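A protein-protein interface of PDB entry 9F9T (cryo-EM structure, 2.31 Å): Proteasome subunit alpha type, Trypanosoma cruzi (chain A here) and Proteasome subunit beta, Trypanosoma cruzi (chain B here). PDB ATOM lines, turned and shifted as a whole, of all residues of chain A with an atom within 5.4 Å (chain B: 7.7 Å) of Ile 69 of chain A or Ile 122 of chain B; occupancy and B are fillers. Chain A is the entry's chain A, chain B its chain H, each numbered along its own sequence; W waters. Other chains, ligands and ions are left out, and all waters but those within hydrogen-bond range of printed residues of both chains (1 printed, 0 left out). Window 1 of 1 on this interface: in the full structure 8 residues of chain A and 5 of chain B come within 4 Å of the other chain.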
ATOM      1  N   HIS A  67      -4.800   6.168 -29.073  1.00  0.00           N
ATOM      2  CA  HIS A  67      -4.180   7.469 -29.144  1.00  0.00           C
ATOM      3  C   HIS A  67      -3.467   7.751 -27.844  1.00  0.00           C
ATOM      4  O   HIS A  67      -3.873   7.268 -26.821  1.00  0.00           O
ATOM      5  CB  HIS A  67      -5.211   8.562 -29.395  1.00  0.00           C
ATOM      6  CG  HIS A  67      -5.943   8.421 -30.661  1.00  0.00           C
ATOM      7  ND1 HIS A  67      -5.463   8.945 -31.837  1.00  0.00           N
ATOM      8  CD2 HIS A  67      -7.051   7.730 -30.970  1.00  0.00           C
ATOM      9  CE1 HIS A  67      -6.280   8.564 -32.806  1.00  0.00           C
ATOM     10  NE2 HIS A  67      -7.303   7.885 -32.301  1.00  0.00           N
ATOM     11  N   ASN A  68      -2.419   8.549 -27.897  1.00  0.00           N
ATOM     12  CA  ASN A  68      -1.848   9.050 -26.670  1.00  0.00           C
ATOM     13  C   ASN A  68      -2.543  10.303 -26.229  1.00  0.00           C
ATOM     14  O   ASN A  68      -2.667  11.240 -27.015  1.00  0.00           O
ATOM     15  CB  ASN A  68      -0.377   9.371 -26.790  1.00  0.00           C
ATOM     16  CG  ASN A  68       0.392   8.089 -26.889  1.00  0.00           C
ATOM     17  OD1 ASN A  68       0.389   7.410 -27.910  1.00  0.00           O
ATOM     18  ND2 ASN A  68       1.038   7.730 -25.799  1.00  0.00           N
ATOM     19  N   ILE A  69      -2.851  10.383 -24.950  1.00  0.00           N
ATOM     20  CA  ILE A  69      -3.299  11.635 -24.410  1.00  0.00           C
ATOM     21  C   ILE A  69      -2.106  12.433 -23.956  1.00  0.00           C
ATOM     22  O   ILE A  69      -2.082  13.656 -24.055  1.00  0.00           O
ATOM     23  CB  ILE A  69      -4.281  11.405 -23.260  1.00  0.00           C
ATOM     24  CG1 ILE A  69      -5.426  10.541 -23.736  1.00  0.00           C
ATOM     25  CG2 ILE A  69      -4.795  12.731 -22.745  1.00  0.00           C
ATOM     26  CD1 ILE A  69      -6.108  11.180 -24.943  1.00  0.00           C
ATOM     27  N   ASN A  70      -1.109  11.730 -23.450  1.00  0.00           N
ATOM     28  CA  ASN A  70       0.176  12.341 -23.211  1.00  0.00           C
ATOM     29  C   ASN A  70       1.179  11.204 -23.188  1.00  0.00           C
ATOM     30  O   ASN A  70       0.889  10.160 -23.710  1.00  0.00           O
ATOM     31  CB  ASN A  70       0.095  13.135 -21.921  1.00  0.00           C
ATOM     32  CG  ASN A  70       0.041  12.250 -20.694  1.00  0.00           C
ATOM     33  OD1 ASN A  70      -0.039  11.020 -20.782  1.00  0.00           O
ATOM     34  ND2 ASN A  70       0.141  12.871 -19.544  1.00  0.00           N
ATOM     35  N   LYS A  71       2.378  11.380 -22.711  1.00  0.00           N
ATOM     36  CA  LYS A  71       3.352  10.291 -22.814  1.00  0.00           C
ATOM     37  C   LYS A  71       2.815   9.001 -22.166  1.00  0.00           C
ATOM     38  O   LYS A  71       2.983   7.893 -22.706  1.00  0.00           O
ATOM     39  CB  LYS A  71       4.636  10.705 -22.097  1.00  0.00           C
ATOM     40  CG  LYS A  71       5.902  10.361 -22.842  1.00  0.00           C
ATOM     41  CD  LYS A  71       7.167  10.801 -22.101  1.00  0.00           C
ATOM     42  CE  LYS A  71       8.425  10.329 -22.811  1.00  0.00           C
ATOM     43  NZ  LYS A  71       9.599  10.298 -21.908  1.00  0.00           N
ATOM     44  N   ILE A  73      -0.507   8.190 -20.897  1.00  0.00           N
ATOM     45  CA  ILE A  73      -1.896   7.797 -20.912  1.00  0.00           C
ATOM     46  C   ILE A  73      -2.298   7.523 -22.348  1.00  0.00           C
ATOM     47  O   ILE A  73      -2.099   8.365 -23.198  1.00  0.00           O
ATOM     48  CB  ILE A  73      -2.739   8.923 -20.289  1.00  0.00           C
ATOM     49  CG1 ILE A  73      -2.485   9.133 -18.809  1.00  0.00           C
ATOM     50  CG2 ILE A  73      -4.221   8.748 -20.475  1.00  0.00           C
ATOM     51  CD1 ILE A  73      -3.272  10.289 -18.285  1.00  0.00           C
ATOM     52  N   GLY A  74      -2.969   6.406 -22.576  1.00  0.00           N
ATOM     53  CA  GLY A  74      -3.452   6.036 -23.884  1.00  0.00           C
ATOM     54  C   GLY A  74      -4.949   5.859 -23.825  1.00  0.00           C
ATOM     55  O   GLY A  74      -5.487   5.833 -22.730  1.00  0.00           O
ATOM     56  N   THR A  75      -5.617   5.975 -24.976  1.00  0.00           N
ATOM     57  CA  THR A  75      -7.049   5.776 -25.083  1.00  0.00           C
ATOM     58  C   THR A  75      -7.318   4.784 -26.187  1.00  0.00           C
ATOM     59  O   THR A  75      -6.490   4.551 -27.056  1.00  0.00           O
ATOM     60  CB  THR A  75      -7.931   6.971 -25.486  1.00  0.00           C
ATOM     61  OG1 THR A  75      -7.393   7.851 -26.471  1.00  0.00           O
ATOM     62  CG2 THR A  75      -8.268   7.845 -24.307  1.00  0.00           C
ATOM     63  N   VAL A  88     -10.479  13.027 -27.885  1.00  0.00           N
ATOM     64  CA  VAL A  88      -9.024  12.940 -27.749  1.00  0.00           C
ATOM     65  C   VAL A  88      -8.385  14.315 -27.655  1.00  0.00           C
ATOM     66  O   VAL A  88      -7.568  14.556 -26.763  1.00  0.00           O
ATOM     67  CB  VAL A  88      -8.405  12.154 -28.892  1.00  0.00           C
ATOM     68  CG1 VAL A  88      -6.897  12.236 -28.947  1.00  0.00           C
ATOM     69  CG2 VAL A  88      -8.844  10.696 -28.826  1.00  0.00           C
ATOM     70  N   ALA A  91      -9.394  15.908 -24.088  1.00  0.00           N
ATOM     71  CA  ALA A  91      -8.517  15.232 -23.180  1.00  0.00           C
ATOM     72  C   ALA A  91      -7.107  15.773 -23.286  1.00  0.00           C
ATOM     73  O   ALA A  91      -6.465  15.822 -22.258  1.00  0.00           O
ATOM     74  CB  ALA A  91      -8.570  13.768 -23.465  1.00  0.00           C
ATOM     75  N   ARG A  92      -6.570  16.098 -24.491  1.00  0.00           N
ATOM     76  CA  ARG A  92      -5.141  16.487 -24.616  1.00  0.00           C
ATOM     77  C   ARG A  92      -4.971  17.870 -24.040  1.00  0.00           C
ATOM     78  O   ARG A  92      -4.015  18.139 -23.311  1.00  0.00           O
ATOM     79  CB  ARG A  92      -4.616  16.438 -26.040  1.00  0.00           C
ATOM     80  CG  ARG A  92      -4.195  15.034 -26.467  1.00  0.00           C
ATOM     81  CD  ARG A  92      -4.055  14.859 -27.940  1.00  0.00           C
ATOM     82  NE  ARG A  92      -3.484  13.592 -28.258  1.00  0.00           N
ATOM     83  CZ  ARG A  92      -3.353  13.149 -29.510  1.00  0.00           C
ATOM     84  NH1 ARG A  92      -3.752  13.907 -30.502  1.00  0.00           N
ATOM     85  NH2 ARG A  92      -2.809  11.970 -29.768  1.00  0.00           N
ATOM     86  N   ALA A  95      -5.177  17.676 -20.333  1.00  0.00           N
ATOM     87  CA  ALA A  95      -3.978  17.155 -19.728  1.00  0.00           C
ATOM     88  C   ALA A  95      -2.906  18.234 -19.652  1.00  0.00           C
ATOM     89  O   ALA A  95      -2.160  18.297 -18.684  1.00  0.00           O
ATOM     90  CB  ALA A  95      -3.521  15.952 -20.434  1.00  0.00           C
ATOM     91  N   LEU A 111      -7.829  12.367 -15.091  1.00  0.00           N
ATOM     92  CA  LEU A 111      -8.164  12.642 -16.469  1.00  0.00           C
ATOM     93  C   LEU A 111      -9.576  12.150 -16.819  1.00  0.00           C
ATOM     94  O   LEU A 111     -10.418  12.880 -17.362  1.00  0.00           O
ATOM     95  CB  LEU A 111      -7.127  12.011 -17.413  1.00  0.00           C
ATOM     96  CG  LEU A 111      -7.527  12.234 -18.874  1.00  0.00           C
ATOM     97  CD1 LEU A 111      -7.343  13.682 -19.292  1.00  0.00           C
ATOM     98  CD2 LEU A 111      -6.830  11.326 -19.830  1.00  0.00           C
ATOM     99  N   PHE A 137      -9.565   4.736 -21.025  1.00  0.00           N
ATOM    100  CA  PHE A 137      -8.249   5.276 -20.681  1.00  0.00           C
ATOM    101  C   PHE A 137      -7.411   4.221 -19.954  1.00  0.00           C
ATOM    102  O   PHE A 137      -7.902   3.472 -19.141  1.00  0.00           O
ATOM    103  CB  PHE A 137      -8.368   6.490 -19.784  1.00  0.00           C
ATOM    104  CG  PHE A 137      -9.068   7.640 -20.427  1.00  0.00           C
ATOM    105  CD1 PHE A 137      -8.389   8.506 -21.250  1.00  0.00           C
ATOM    106  CD2 PHE A 137     -10.451   7.776 -20.331  1.00  0.00           C
ATOM    107  CE1 PHE A 137      -9.045   9.494 -21.968  1.00  0.00           C
ATOM    108  CE2 PHE A 137     -11.105   8.799 -20.995  1.00  0.00           C
ATOM    109  CZ  PHE A 137     -10.413   9.649 -21.822  1.00  0.00           C
ATOM    110  N   ASN B 115       5.653  23.383 -22.290  1.00  0.00           N
ATOM    111  CA  ASN B 115       4.259  23.011 -22.288  1.00  0.00           C
ATOM    112  C   ASN B 115       3.774  22.924 -23.739  1.00  0.00           C
ATOM    113  O   ASN B 115       3.220  21.913 -24.145  1.00  0.00           O
ATOM    114  CB  ASN B 115       3.462  23.937 -21.353  1.00  0.00           C
ATOM    115  CG  ASN B 115       1.951  23.643 -21.337  1.00  0.00           C
ATOM    116  OD1 ASN B 115       1.118  24.429 -21.821  1.00  0.00           O
ATOM    117  ND2 ASN B 115       1.567  22.505 -20.790  1.00  0.00           N
ATOM    118  N   TYR B 116       4.080  23.945 -24.559  1.00  0.00           N
ATOM    119  CA  TYR B 116       3.718  23.966 -25.968  1.00  0.00           C
ATOM    120  C   TYR B 116       4.361  22.857 -26.768  1.00  0.00           C
ATOM    121  O   TYR B 116       3.739  22.409 -27.719  1.00  0.00           O
ATOM    122  CB  TYR B 116       4.082  25.242 -26.726  1.00  0.00           C
ATOM    123  CG  TYR B 116       3.335  26.475 -26.261  1.00  0.00           C
ATOM    124  CD1 TYR B 116       1.974  26.418 -25.967  1.00  0.00           C
ATOM    125  CD2 TYR B 116       3.960  27.718 -26.163  1.00  0.00           C
ATOM    126  CE1 TYR B 116       1.263  27.555 -25.596  1.00  0.00           C
ATOM    127  CE2 TYR B 116       3.273  28.848 -25.748  1.00  0.00           C
ATOM    128  CZ  TYR B 116       1.922  28.766 -25.441  1.00  0.00           C
ATOM    129  OH  TYR B 116       1.203  29.862 -25.061  1.00  0.00           O
ATOM    130  N   LEU B 117       5.625  22.538 -26.507  1.00  0.00           N
ATOM    131  CA  LEU B 117       6.306  21.564 -27.317  1.00  0.00           C
ATOM    132  C   LEU B 117       5.817  20.177 -27.008  1.00  0.00           C
ATOM    133  O   LEU B 117       5.855  19.320 -27.871  1.00  0.00           O
ATOM    134  CB  LEU B 117       7.799  21.574 -27.010  1.00  0.00           C
ATOM    135  CG  LEU B 117       8.582  22.755 -27.556  1.00  0.00           C
ATOM    136  CD1 LEU B 117       9.919  22.853 -26.858  1.00  0.00           C
ATOM    137  CD2 LEU B 117       8.757  22.644 -29.074  1.00  0.00           C
ATOM    138  N   GLU B 118       5.408  19.907 -25.779  1.00  0.00           N
ATOM    139  CA  GLU B 118       4.943  18.557 -25.421  1.00  0.00           C
ATOM    140  C   GLU B 118       3.594  18.245 -26.100  1.00  0.00           C
ATOM    141  O   GLU B 118       3.458  17.152 -26.650  1.00  0.00           O
ATOM    142  CB  GLU B 118       4.996  18.479 -23.892  1.00  0.00           C
ATOM    143  CG  GLU B 118       4.220  17.384 -23.187  1.00  0.00           C
ATOM    144  CD  GLU B 118       4.280  17.579 -21.660  1.00  0.00           C
ATOM    145  OE1 GLU B 118       3.721  18.605 -21.154  1.00  0.00           O
ATOM    146  OE2 GLU B 118       4.921  16.736 -20.959  1.00  0.00           O
ATOM    147  N   SER B 119       2.682  19.224 -26.099  1.00  0.00           N
ATOM    148  CA  SER B 119       1.454  19.230 -26.883  1.00  0.00           C
ATOM    149  C   SER B 119       1.699  19.000 -28.355  1.00  0.00           C
ATOM    150  O   SER B 119       1.130  18.129 -28.952  1.00  0.00           O
ATOM    151  CB  SER B 119       0.741  20.515 -26.794  1.00  0.00           C
ATOM    152  OG  SER B 119       0.543  20.985 -25.485  1.00  0.00           O
ATOM    153  N   TYR B 120       2.609  19.736 -28.944  1.00  0.00           N
ATOM    154  CA  TYR B 120       2.920  19.591 -30.359  1.00  0.00           C
ATOM    155  C   TYR B 120       3.467  18.216 -30.655  1.00  0.00           C
ATOM    156  O   TYR B 120       3.098  17.635 -31.643  1.00  0.00           O
ATOM    157  CB  TYR B 120       3.899  20.711 -30.766  1.00  0.00           C
ATOM    158  CG  TYR B 120       4.304  20.616 -32.224  1.00  0.00           C
ATOM    159  CD1 TYR B 120       3.411  20.981 -33.197  1.00  0.00           C
ATOM    160  CD2 TYR B 120       5.551  20.119 -32.638  1.00  0.00           C
ATOM    161  CE1 TYR B 120       3.757  20.926 -34.532  1.00  0.00           C
ATOM    162  CE2 TYR B 120       5.892  20.040 -33.983  1.00  0.00           C
ATOM    163  CZ  TYR B 120       4.983  20.452 -34.924  1.00  0.00           C
ATOM    164  OH  TYR B 120       5.067  20.330 -36.274  1.00  0.00           O
ATOM    165  N   GLU B 121       4.361  17.687 -29.835  1.00  0.00           N
ATOM    166  CA  GLU B 121       4.846  16.326 -30.069  1.00  0.00           C
ATOM    167  C   GLU B 121       3.773  15.231 -29.954  1.00  0.00           C
ATOM    168  O   GLU B 121       3.872  14.204 -30.600  1.00  0.00           O
ATOM    169  CB  GLU B 121       5.943  16.139 -29.053  1.00  0.00           C
ATOM    170  CG  GLU B 121       6.630  14.824 -29.081  1.00  0.00           C
ATOM    171  CD  GLU B 121       7.866  14.889 -28.176  1.00  0.00           C
ATOM    172  OE1 GLU B 121       8.249  16.027 -27.730  1.00  0.00           O
ATOM    173  OE2 GLU B 121       8.432  13.799 -27.877  1.00  0.00           O
ATOM    174  N   ILE B 122       2.729  15.423 -29.140  1.00  0.00           N
ATOM    175  CA  ILE B 122       1.695  14.416 -29.065  1.00  0.00           C
ATOM    176  C   ILE B 122       0.825  14.411 -30.327  1.00  0.00           C
ATOM    177  O   ILE B 122       0.389  13.347 -30.788  1.00  0.00           O
ATOM    178  CB  ILE B 122       0.822  14.677 -27.808  1.00  0.00           C
ATOM    179  CG1 ILE B 122       1.474  14.259 -26.497  1.00  0.00           C
ATOM    180  CG2 ILE B 122      -0.518  13.997 -27.906  1.00  0.00           C
ATOM    181  CD1 ILE B 122       0.958  15.130 -25.363  1.00  0.00           C
ATOM    182  N   ASP B 123       0.466  15.601 -30.794  1.00  0.00           N
ATOM    183  CA  ASP B 123      -0.262  15.798 -32.026  1.00  0.00           C
ATOM    184  C   ASP B 123       0.499  15.163 -33.176  1.00  0.00           C
ATOM    185  O   ASP B 123       0.192  14.070 -33.667  1.00  0.00           O
ATOM    186  CB  ASP B 123      -0.468  17.290 -32.233  1.00  0.00           C
ATOM    187  CG  ASP B 123      -1.820  17.697 -32.797  1.00  0.00           C
ATOM    188  OD1 ASP B 123      -2.836  16.966 -32.542  1.00  0.00           O
ATOM    189  OD2 ASP B 123      -1.862  18.766 -33.480  1.00  0.00           O
ATOM    190  N   THR B 124       1.616  15.762 -33.524  1.00  0.00           N
ATOM    191  CA  THR B 124       2.440  15.235 -34.598  1.00  0.00           C
ATOM    192  C   THR B 124       2.867  13.775 -34.425  1.00  0.00           C
ATOM    193  O   THR B 124       3.160  13.142 -35.434  1.00  0.00           O
ATOM    194  CB  THR B 124       3.692  16.110 -34.730  1.00  0.00           C
ATOM    195  OG1 THR B 124       4.436  16.118 -33.513  1.00  0.00           O
ATOM    196  CG2 THR B 124       3.316  17.523 -35.057  1.00  0.00           C
ATOM    197  N   SER B 125       3.014  13.285 -33.188  1.00  0.00           N
ATOM    198  CA  SER B 125       3.562  11.972 -32.873  1.00  0.00           C
ATOM    199  C   SER B 125       5.038  11.855 -33.238  1.00  0.00           C
ATOM    200  O   SER B 125       5.496  10.739 -33.479  1.00  0.00           O
ATOM    201  CB  SER B 125       2.835  10.813 -33.567  1.00  0.00           C
ATOM    202  OG  SER B 125       1.450  10.730 -33.251  1.00  0.00           O
ATOM    203  N   LYS B 126       5.777  12.969 -33.307  1.00  0.00           N
ATOM    204  CA  LYS B 126       7.164  12.951 -33.754  1.00  0.00           C
ATOM    205  C   LYS B 126       8.031  13.742 -32.782  1.00  0.00           C
ATOM    206  O   LYS B 126       7.572  14.655 -32.107  1.00  0.00           O
ATOM    207  CB  LYS B 126       7.276  13.567 -35.155  1.00  0.00           C
ATOM    208  CG  LYS B 126       6.605  12.750 -36.251  1.00  0.00           C
ATOM    209  CD  LYS B 126       6.575  13.420 -37.621  1.00  0.00           C
ATOM    210  CE  LYS B 126       7.933  13.467 -38.294  1.00  0.00           C
ATOM    211  NZ  LYS B 126       7.831  13.663 -39.763  1.00  0.00           N
ATOM    212  N   VAL B 128      10.581  16.715 -31.772  1.00  0.00           N
ATOM    213  CA  VAL B 128      10.429  18.049 -32.278  1.00  0.00           C
ATOM    214  C   VAL B 128      11.780  18.574 -32.646  1.00  0.00           C
ATOM    215  O   VAL B 128      12.770  18.167 -32.072  1.00  0.00           O
ATOM    216  CB  VAL B 128       9.654  18.934 -31.307  1.00  0.00           C
ATOM    217  CG1 VAL B 128       8.768  18.056 -30.444  1.00  0.00           C
ATOM    218  CG2 VAL B 128      10.479  19.775 -30.396  1.00  0.00           C
HETATM  219  O   HOH W   1       3.462  14.152 -22.459  1.00  0.00           O
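Of the 14 printed residues of chain A, 4 touch a printed residue of chain B. Along chain B the printed residues that touch a printed residue of chain A span positions 122 to 123. Among the printed residues, 5 pairs touch across the chains. Among the printed residues, Asp or Glu carboxylates within 4 Å of a Lys or Arg side-chain nitrogen of the other chain: Arg 92 of chain A with Asp 123 of chain B (3.8 Å).
Water W1 bridges the backbone NH of Lys 71 of chain A and the side-chain carboxylate of Glu 118 of chain B.
NH1 of Arg 92 of chain A lies within salt-bridge range of OD1 of Asp 123 of chain B (3.8 Å).
Asn 68 of chain A touches Ile 122 of chain B. Ile 122 of chain B touches Ile 69 of chain A. Asn 70 of chain A touches Ile 122 of chain B. Ile 122 of chain B touches Arg 92 of chain A.
Of chain B, only Ile 122 (3.6 Å) comes within 4 Å of Ile 69 of chain A. Of chain A, only Asn 68 (3.6 Å), Ile 69 (3.6 Å), Asn 70 (3.6 Å) and Arg 92 (3.0 Å) come within 4 Å of Ile 122 of chain B. Of the printed residues of chain A, Asp 123 of chain B touches Arg 92. Printed residues of chain B within 4 Å of Asn 68 of chain A: Ile 122. Of the printed residues of chain B, Asn 70 of chain A touches Ile 122 (3.6 Å). Leu 117 of chain B touches none of the printed residues of chain A. Ala 91 of chain A touches none of the printed residues of chain B. The nearest residue of chain B that does not touch Ile 69 of chain A is Glu 118 of chain B (7.0 Å). The nearest residue of chain A that does not touch Ile 122 of chain B is Lys 71 of chain A (4.8 Å).
The side-chain amide oxygen (OD1) of Asn 70 of chain A is in hydrogen-bond range of the backbone NH (N) of Ile 73 of chain A. ND2 of Asn 68 of chain A sits at hydrogen-bond distance from O of Asn 70 of chain A (3.2 Å). The guanidinium group (NE) of Arg 92 of chain A lies within hydrogen-bond range of the backbone carbonyl oxygen (O) of Asn 68 of chain A (2.8 Å).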
